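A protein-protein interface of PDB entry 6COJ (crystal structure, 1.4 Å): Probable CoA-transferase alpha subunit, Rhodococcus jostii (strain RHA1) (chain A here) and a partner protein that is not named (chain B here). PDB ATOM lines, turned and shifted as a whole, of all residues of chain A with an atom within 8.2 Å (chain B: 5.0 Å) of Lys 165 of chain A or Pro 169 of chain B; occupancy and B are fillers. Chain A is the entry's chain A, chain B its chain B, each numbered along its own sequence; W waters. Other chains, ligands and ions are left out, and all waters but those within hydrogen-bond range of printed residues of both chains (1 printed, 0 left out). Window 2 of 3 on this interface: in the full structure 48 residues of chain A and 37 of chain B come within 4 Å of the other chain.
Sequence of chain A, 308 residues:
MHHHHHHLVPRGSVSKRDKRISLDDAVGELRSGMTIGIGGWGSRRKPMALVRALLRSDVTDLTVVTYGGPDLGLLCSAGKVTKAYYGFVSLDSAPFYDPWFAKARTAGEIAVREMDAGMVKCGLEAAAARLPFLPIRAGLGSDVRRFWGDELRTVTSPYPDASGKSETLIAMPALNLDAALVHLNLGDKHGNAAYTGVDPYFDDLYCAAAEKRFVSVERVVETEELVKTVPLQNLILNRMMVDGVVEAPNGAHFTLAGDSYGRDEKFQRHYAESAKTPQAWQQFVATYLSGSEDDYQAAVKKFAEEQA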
ATOM      1  N   ARG A 137       2.740  37.388   6.449  1.00  0.00           N
ATOM      2  CA  ARG A 137       4.109  37.187   6.904  1.00  0.00           C
ATOM      3  C   ARG A 137       4.444  38.122   8.062  1.00  0.00           C
ATOM      4  O   ARG A 137       5.090  37.706   9.034  1.00  0.00           O
ATOM      5  CB  ARG A 137       5.072  37.422   5.742  1.00  0.00           C
ATOM      6  CG  ARG A 137       6.475  36.931   5.994  1.00  0.00           C
ATOM      7  CD  ARG A 137       7.347  37.016   4.748  1.00  0.00           C
ATOM      8  NE  ARG A 137       6.547  36.926   3.541  1.00  0.00           N
ATOM      9  CZ  ARG A 137       6.415  35.811   2.843  1.00  0.00           C
ATOM     10  NH1 ARG A 137       5.661  35.792   1.743  1.00  0.00           N
ATOM     11  NH2 ARG A 137       7.021  34.709   3.269  1.00  0.00           N
ATOM     12  N   LEU A 140       5.875  37.589  12.080  1.00  0.00           N
ATOM     13  CA  LEU A 140       6.762  36.457  12.329  1.00  0.00           C
ATOM     14  C   LEU A 140       8.119  36.935  12.815  1.00  0.00           C
ATOM     15  O   LEU A 140       8.703  37.872  12.259  1.00  0.00           O
ATOM     16  CB  LEU A 140       6.965  35.653  11.047  1.00  0.00           C
ATOM     17  CG  LEU A 140       5.857  34.737  10.552  1.00  0.00           C
ATOM     18  CD1 LEU A 140       6.286  34.194   9.207  1.00  0.00           C
ATOM     19  CD2 LEU A 140       5.595  33.582  11.521  1.00  0.00           C
ATOM     20  N   THR A 156      -0.354  26.872   8.894  1.00  0.00           N
ATOM     21  CA  THR A 156       0.565  26.256   7.944  1.00  0.00           C
ATOM     22  C   THR A 156      -0.114  26.032   6.597  1.00  0.00           C
ATOM     23  O   THR A 156      -1.260  25.581   6.532  1.00  0.00           O
ATOM     24  CB  THR A 156       1.082  24.938   8.512  1.00  0.00           C
ATOM     25  OG1 THR A 156       1.799  25.216   9.717  1.00  0.00           O
ATOM     26  CG2 THR A 156       2.023  24.253   7.532  1.00  0.00           C
ATOM     27  N   SER A 157       0.595  26.371   5.528  1.00  0.00           N
ATOM     28  CA  SER A 157       0.077  26.149   4.187  1.00  0.00           C
ATOM     29  C   SER A 157      -0.177  24.666   3.946  1.00  0.00           C
ATOM     30  O   SER A 157       0.703  23.841   4.226  1.00  0.00           O
ATOM     31  CB  SER A 157       1.088  26.625   3.157  1.00  0.00           C
ATOM     32  OG  SER A 157       0.606  26.360   1.851  1.00  0.00           O
ATOM     33  N   TYR A 159      -0.111  23.531   1.061  1.00  0.00           N
ATOM     34  CA  TYR A 159       0.717  23.289  -0.116  1.00  0.00           C
ATOM     35  C   TYR A 159       2.158  23.574   0.253  1.00  0.00           C
ATOM     36  O   TYR A 159       2.482  24.719   0.597  1.00  0.00           O
ATOM     37  CB  TYR A 159       0.297  24.209  -1.263  1.00  0.00           C
ATOM     38  CG  TYR A 159      -1.183  24.242  -1.514  1.00  0.00           C
ATOM     39  CD1 TYR A 159      -1.831  23.164  -2.100  1.00  0.00           C
ATOM     40  CD2 TYR A 159      -1.933  25.344  -1.151  1.00  0.00           C
ATOM     41  CE1 TYR A 159      -3.182  23.187  -2.323  1.00  0.00           C
ATOM     42  CE2 TYR A 159      -3.288  25.384  -1.375  1.00  0.00           C
ATOM     43  CZ  TYR A 159      -3.911  24.305  -1.952  1.00  0.00           C
ATOM     44  OH  TYR A 159      -5.260  24.342  -2.174  1.00  0.00           O
ATOM     45  N   PRO A 160       3.051  22.593   0.224  1.00  0.00           N
ATOM     46  CA  PRO A 160       4.469  22.897   0.416  1.00  0.00           C
ATOM     47  C   PRO A 160       4.983  23.731  -0.744  1.00  0.00           C
ATOM     48  O   PRO A 160       4.426  23.727  -1.846  1.00  0.00           O
ATOM     49  CB  PRO A 160       5.130  21.509   0.416  1.00  0.00           C
ATOM     50  CG  PRO A 160       4.009  20.554   0.726  1.00  0.00           C
ATOM     51  CD  PRO A 160       2.811  21.153   0.053  1.00  0.00           C
ATOM     52  N   ASP A 161       6.058  24.467  -0.483  1.00  0.00           N
ATOM     53  CA  ASP A 161       6.756  25.153  -1.556  1.00  0.00           C
ATOM     54  C   ASP A 161       7.443  24.116  -2.452  1.00  0.00           C
ATOM     55  O   ASP A 161       7.420  22.909  -2.185  1.00  0.00           O
ATOM     56  CB  ASP A 161       7.722  26.191  -0.979  1.00  0.00           C
ATOM     57  CG  ASP A 161       7.003  27.360  -0.276  1.00  0.00           C
ATOM     58  OD1 ASP A 161       5.756  27.353  -0.178  1.00  0.00           O
ATOM     59  OD2 ASP A 161       7.690  28.297   0.192  1.00  0.00           O
ATOM     60  N   ALA A 162       8.073  24.596  -3.528  1.00  0.00           N
ATOM     61  CA  ALA A 162       8.705  23.688  -4.483  1.00  0.00           C
ATOM     62  C   ALA A 162       9.723  22.771  -3.810  1.00  0.00           C
ATOM     63  O   ALA A 162       9.826  21.588  -4.159  1.00  0.00           O
ATOM     64  CB  ALA A 162       9.349  24.487  -5.615  1.00  0.00           C
ATOM     65  N   SER A 163      10.469  23.292  -2.831  1.00  0.00           N
ATOM     66  CA  SER A 163      11.507  22.519  -2.153  1.00  0.00           C
ATOM     67  C   SER A 163      10.950  21.401  -1.283  1.00  0.00           C
ATOM     68  O   SER A 163      11.724  20.557  -0.818  1.00  0.00           O
ATOM     69  CB  SER A 163      12.357  23.440  -1.278  1.00  0.00           C
ATOM     70  OG  SER A 163      11.620  23.881  -0.149  1.00  0.00           O
ATOM     71  N   GLY A 164       9.644  21.381  -1.041  1.00  0.00           N
ATOM     72  CA  GLY A 164       9.046  20.414  -0.151  1.00  0.00           C
ATOM     73  C   GLY A 164       8.787  20.930   1.244  1.00  0.00           C
ATOM     74  O   GLY A 164       8.238  20.188   2.064  1.00  0.00           O
ATOM     75  N   LYS A 165       9.134  22.180   1.531  1.00  0.00           N
ATOM     76  CA  LYS A 165       8.916  22.760   2.850  1.00  0.00           C
ATOM     77  C   LYS A 165       7.624  23.561   2.858  1.00  0.00           C
ATOM     78  O   LYS A 165       7.355  24.333   1.937  1.00  0.00           O
ATOM     79  CB  LYS A 165      10.055  23.701   3.230  1.00  0.00           C
ATOM     80  CG  LYS A 165      11.393  23.047   3.485  1.00  0.00           C
ATOM     81  CD  LYS A 165      12.388  24.129   3.870  1.00  0.00           C
ATOM     82  CE  LYS A 165      13.744  23.557   4.191  1.00  0.00           C
ATOM     83  NZ  LYS A 165      14.393  23.025   2.964  1.00  0.00           N
ATOM     84  N   SER A 166       6.847  23.406   3.921  1.00  0.00           N
ATOM     85  CA  SER A 166       5.581  24.116   4.061  1.00  0.00           C
ATOM     86  C   SER A 166       5.779  25.391   4.868  1.00  0.00           C
ATOM     87  O   SER A 166       6.428  25.382   5.920  1.00  0.00           O
ATOM     88  CB  SER A 166       4.561  23.230   4.770  1.00  0.00           C
ATOM     89  OG  SER A 166       4.354  22.036   4.030  1.00  0.00           O
ATOM     90  N   GLU A 167       5.213  26.483   4.374  1.00  0.00           N
ATOM     91  CA  GLU A 167       5.325  27.760   5.059  1.00  0.00           C
ATOM     92  C   GLU A 167       4.335  27.829   6.204  1.00  0.00           C
ATOM     93  O   GLU A 167       3.168  27.459   6.057  1.00  0.00           O
ATOM     94  CB  GLU A 167       4.981  28.885   4.095  1.00  0.00           C
ATOM     95  CG  GLU A 167       5.974  29.087   3.004  1.00  0.00           C
ATOM     96  CD  GLU A 167       5.809  30.439   2.343  1.00  0.00           C
ATOM     97  OE1 GLU A 167       6.253  30.572   1.188  1.00  0.00           O
ATOM     98  OE2 GLU A 167       5.243  31.356   2.977  1.00  0.00           O
ATOM     99  N   THR A 168       4.799  28.344   7.339  1.00  0.00           N
ATOM    100  CA  THR A 168       3.940  28.642   8.477  1.00  0.00           C
ATOM    101  C   THR A 168       3.908  30.156   8.646  1.00  0.00           C
ATOM    102  O   THR A 168       4.958  30.793   8.777  1.00  0.00           O
ATOM    103  CB  THR A 168       4.451  27.955   9.740  1.00  0.00           C
ATOM    104  OG1 THR A 168       4.391  26.536   9.557  1.00  0.00           O
ATOM    105  CG2 THR A 168       3.591  28.311  10.926  1.00  0.00           C
ATOM    106  N   LEU A 169       2.711  30.725   8.593  1.00  0.00           N
ATOM    107  CA  LEU A 169       2.512  32.167   8.562  1.00  0.00           C
ATOM    108  C   LEU A 169       1.680  32.601   9.763  1.00  0.00           C
ATOM    109  O   LEU A 169       1.058  31.784  10.444  1.00  0.00           O
ATOM    110  CB  LEU A 169       1.802  32.563   7.264  1.00  0.00           C
ATOM    111  CG  LEU A 169       2.576  32.234   5.988  1.00  0.00           C
ATOM    112  CD1 LEU A 169       1.622  31.963   4.830  1.00  0.00           C
ATOM    113  CD2 LEU A 169       3.521  33.371   5.683  1.00  0.00           C
ATOM    114  N   PRO B 166      15.092  28.430   9.801  1.00  0.00           N
ATOM    115  CA  PRO B 166      15.472  27.988   8.452  1.00  0.00           C
ATOM    116  C   PRO B 166      14.573  26.900   7.899  1.00  0.00           C
ATOM    117  O   PRO B 166      14.598  26.651   6.687  1.00  0.00           O
ATOM    118  CB  PRO B 166      16.903  27.472   8.648  1.00  0.00           C
ATOM    119  CG  PRO B 166      16.912  26.986  10.061  1.00  0.00           C
ATOM    120  CD  PRO B 166      16.021  27.936  10.832  1.00  0.00           C
ATOM    121  N   GLU B 167      13.794  26.231   8.744  1.00  0.00           N
ATOM    122  CA  GLU B 167      12.876  25.210   8.265  1.00  0.00           C
ATOM    123  C   GLU B 167      11.593  25.798   7.701  1.00  0.00           C
ATOM    124  O   GLU B 167      10.831  25.073   7.056  1.00  0.00           O
ATOM    125  CB  GLU B 167      12.525  24.239   9.393  1.00  0.00           C
ATOM    126  CG  GLU B 167      13.722  23.516   9.981  1.00  0.00           C
ATOM    127  CD  GLU B 167      13.341  22.624  11.143  1.00  0.00           C
ATOM    128  OE1 GLU B 167      14.233  21.941  11.692  1.00  0.00           O
ATOM    129  OE2 GLU B 167      12.147  22.604  11.508  1.00  0.00           O
ATOM    130  N   ASN B 168      11.338  27.083   7.925  1.00  0.00           N
ATOM    131  CA  ASN B 168      10.088  27.688   7.507  1.00  0.00           C
ATOM    132  C   ASN B 168      10.378  28.700   6.414  1.00  0.00           C
ATOM    133  O   ASN B 168      10.916  29.784   6.701  1.00  0.00           O
ATOM    134  CB  ASN B 168       9.447  28.368   8.711  1.00  0.00           C
ATOM    135  CG  ASN B 168       8.140  29.046   8.379  1.00  0.00           C
ATOM    136  OD1 ASN B 168       7.653  28.989   7.254  1.00  0.00           O
ATOM    137  ND2 ASN B 168       7.550  29.690   9.379  1.00  0.00           N
ATOM    138  N   PRO B 169      10.023  28.402   5.163  1.00  0.00           N
ATOM    139  CA  PRO B 169      10.334  29.331   4.065  1.00  0.00           C
ATOM    140  C   PRO B 169       9.656  30.669   4.190  1.00  0.00           C
ATOM    141  O   PRO B 169       9.989  31.579   3.422  1.00  0.00           O
ATOM    142  CB  PRO B 169       9.857  28.591   2.800  1.00  0.00           C
ATOM    143  CG  PRO B 169       9.636  27.194   3.225  1.00  0.00           C
ATOM    144  CD  PRO B 169       9.336  27.199   4.689  1.00  0.00           C
ATOM    145  N   ALA B 170       8.729  30.835   5.139  1.00  0.00           N
ATOM    146  CA  ALA B 170       8.160  32.155   5.381  1.00  0.00           C
ATOM    147  C   ALA B 170       9.220  33.177   5.768  1.00  0.00           C
ATOM    148  O   ALA B 170       9.000  34.375   5.582  1.00  0.00           O
ATOM    149  CB  ALA B 170       7.094  32.081   6.474  1.00  0.00           C
ATOM    150  N   TYR B 171      10.369  32.733   6.270  1.00  0.00           N
ATOM    151  CA  TYR B 171      11.464  33.606   6.670  1.00  0.00           C
ATOM    152  C   TYR B 171      12.469  33.879   5.556  1.00  0.00           C
ATOM    153  O   TYR B 171      13.465  34.562   5.806  1.00  0.00           O
ATOM    154  CB  TYR B 171      12.227  32.988   7.850  1.00  0.00           C
ATOM    155  CG  TYR B 171      11.533  33.081   9.196  1.00  0.00           C
ATOM    156  CD1 TYR B 171      11.733  34.177  10.020  1.00  0.00           C
ATOM    157  CD2 TYR B 171      10.690  32.072   9.637  1.00  0.00           C
ATOM    158  CE1 TYR B 171      11.116  34.262  11.260  1.00  0.00           C
ATOM    159  CE2 TYR B 171      10.063  32.151  10.875  1.00  0.00           C
ATOM    160  CZ  TYR B 171      10.280  33.250  11.674  1.00  0.00           C
ATOM    161  OH  TYR B 171       9.662  33.329  12.901  1.00  0.00           O
ATOM    162  N   ARG B 172      12.240  33.381   4.336  1.00  0.00           N
ATOM    163  CA  ARG B 172      13.305  33.373   3.336  1.00  0.00           C
ATOM    164  C   ARG B 172      13.636  34.745   2.757  1.00  0.00           C
ATOM    165  O   ARG B 172      14.646  34.865   2.058  1.00  0.00           O
ATOM    166  CB  ARG B 172      12.951  32.409   2.207  1.00  0.00           C
ATOM    167  CG  ARG B 172      11.854  32.881   1.270  1.00  0.00           C
ATOM    168  CD  ARG B 172      11.580  31.764   0.263  1.00  0.00           C
ATOM    169  NE  ARG B 172      10.491  32.065  -0.659  1.00  0.00           N
ATOM    170  CZ  ARG B 172       9.205  32.132  -0.322  1.00  0.00           C
ATOM    171  NH1 ARG B 172       8.825  31.910   0.932  1.00  0.00           N
ATOM    172  NH2 ARG B 172       8.289  32.416  -1.246  1.00  0.00           N
HETATM  173  O   HOH W   1       5.332  31.862  -0.720  1.00  0.00           O
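Of the 7 printed residues of chain B, 6 touch a printed residue of chain A. Hydrophobic or aromatic side chains of chain B that line the printed part of chain A: Pro 169, Ala 170 and Tyr 171. Along chain B the printed residues that touch a printed residue of chain A span positions 167 to 172. Among the printed residues, 15 pairs touch across the chains. Among the printed residues, Asp or Glu carboxylates within 4 Å of a Lys or Arg side-chain nitrogen of the other chain: Asp 161 of chain A with Arg 172 of chain B and Glu 167 of chain A with Arg 172 of chain B.
Printed residues of chain B within 4 Å of Asp 161 of chain A: Pro 169 and Arg 172. Lys 165 of chain A touches just these residues of chain B: Glu 167 and Pro 169. Of the printed residues of chain B, Ser 166 of chain A touches Pro 169 (3.6 Å). Of the printed residues of chain A, Glu 167 of chain B touches Lys 165 (3.7 Å). Of the printed residues of chain A, Pro 169 of chain B touches Asp 161, Lys 165, Ser 166 and Glu 167. The nearest residue of chain B that does not touch Lys 165 of chain A is Pro 166 of chain B (4.1 Å). The nearest printed residue of chain B that does not touch Leu 140 of chain A is Asn 168 of chain B (4.7 Å).
Water W1 lies within hydrogen-bond range of OE1 of Glu 167 of chain A (2.5 Å) and NH2 of Arg 172 of chain B (3.1 Å).
O of Ala 170 of chain B lies within hydrogen-bond range of NH2 of Arg 137 of chain A (3.1 Å). OD2 of Asp 161 of chain A lies within salt-bridge range of NH1 of Arg 172 of chain B, at 3.9 Å. NH1 of Arg 172 of chain B lies within salt-bridge range of OE1 of Glu 167 of chain A, at 2.9 Å. The backbone carbonyl oxygen of Thr 168 of chain A lies within hydrogen-bond range of the side-chain amide nitrogen of Asn 168 of chain B, 2.9 Å away.
The side-chain carboxylate (OE2) of Glu 167 of chain A is in salt-bridge range of the guanidinium group (NH2) of Arg 137 of chain A. The side-chain hydroxyl (OG1) of Thr 156 of chain A lies within hydrogen-bond range of the side-chain hydroxyl (OG1) of Thr 168 of chain A. The backbone carbonyl oxygen of Glu 167 of chain A sits at hydrogen-bond distance from the backbone NH of Ser 157 of chain A, 2.8 Å away. N of Lys 165 of chain A lies close to OG of Ser 163 of chain A (3.4 Å). The side-chain amide oxygen of Asn 168 of chain B lies close to the backbone NH of Ala 170 of chain B, at 3.0 Å. The backbone carbonyl oxygen (O) of Pro 169 of chain B sits at hydrogen-bond distance from the guanidinium group (NH1) of Arg 172 of chain B, at 2.8 Å.
Leu 140 of chain A touches Ala 170 of chain B. Tyr 171 of chain B touches Leu 140 of chain A (OH to C, 3.9 Å). O of Glu 167 of chain B touches CD of Lys 165 of chain A, 3.7 Å away. Pro 169 of chain B touches Lys 165 of chain A (CG to CB, 3.5 Å). O of Ser 166 of chain A touches CD of Pro 169 of chain B, at 3.6 Å. CA of Glu 167 of chain A touches OD1 of Asn 168 of chain B, 3.4 Å away. CG of Glu 167 of chain A touches CB of Pro 169 of chain B (3.9 Å). Glu 167 of chain A touches Ala 170 of chain B. Thr 168 of chain A touches Ala 170 of chain B (O to CB, 3.4 Å). CD2 of Leu 169 of chain A touches CB of Ala 170 of chain B, 3.9 Å away.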
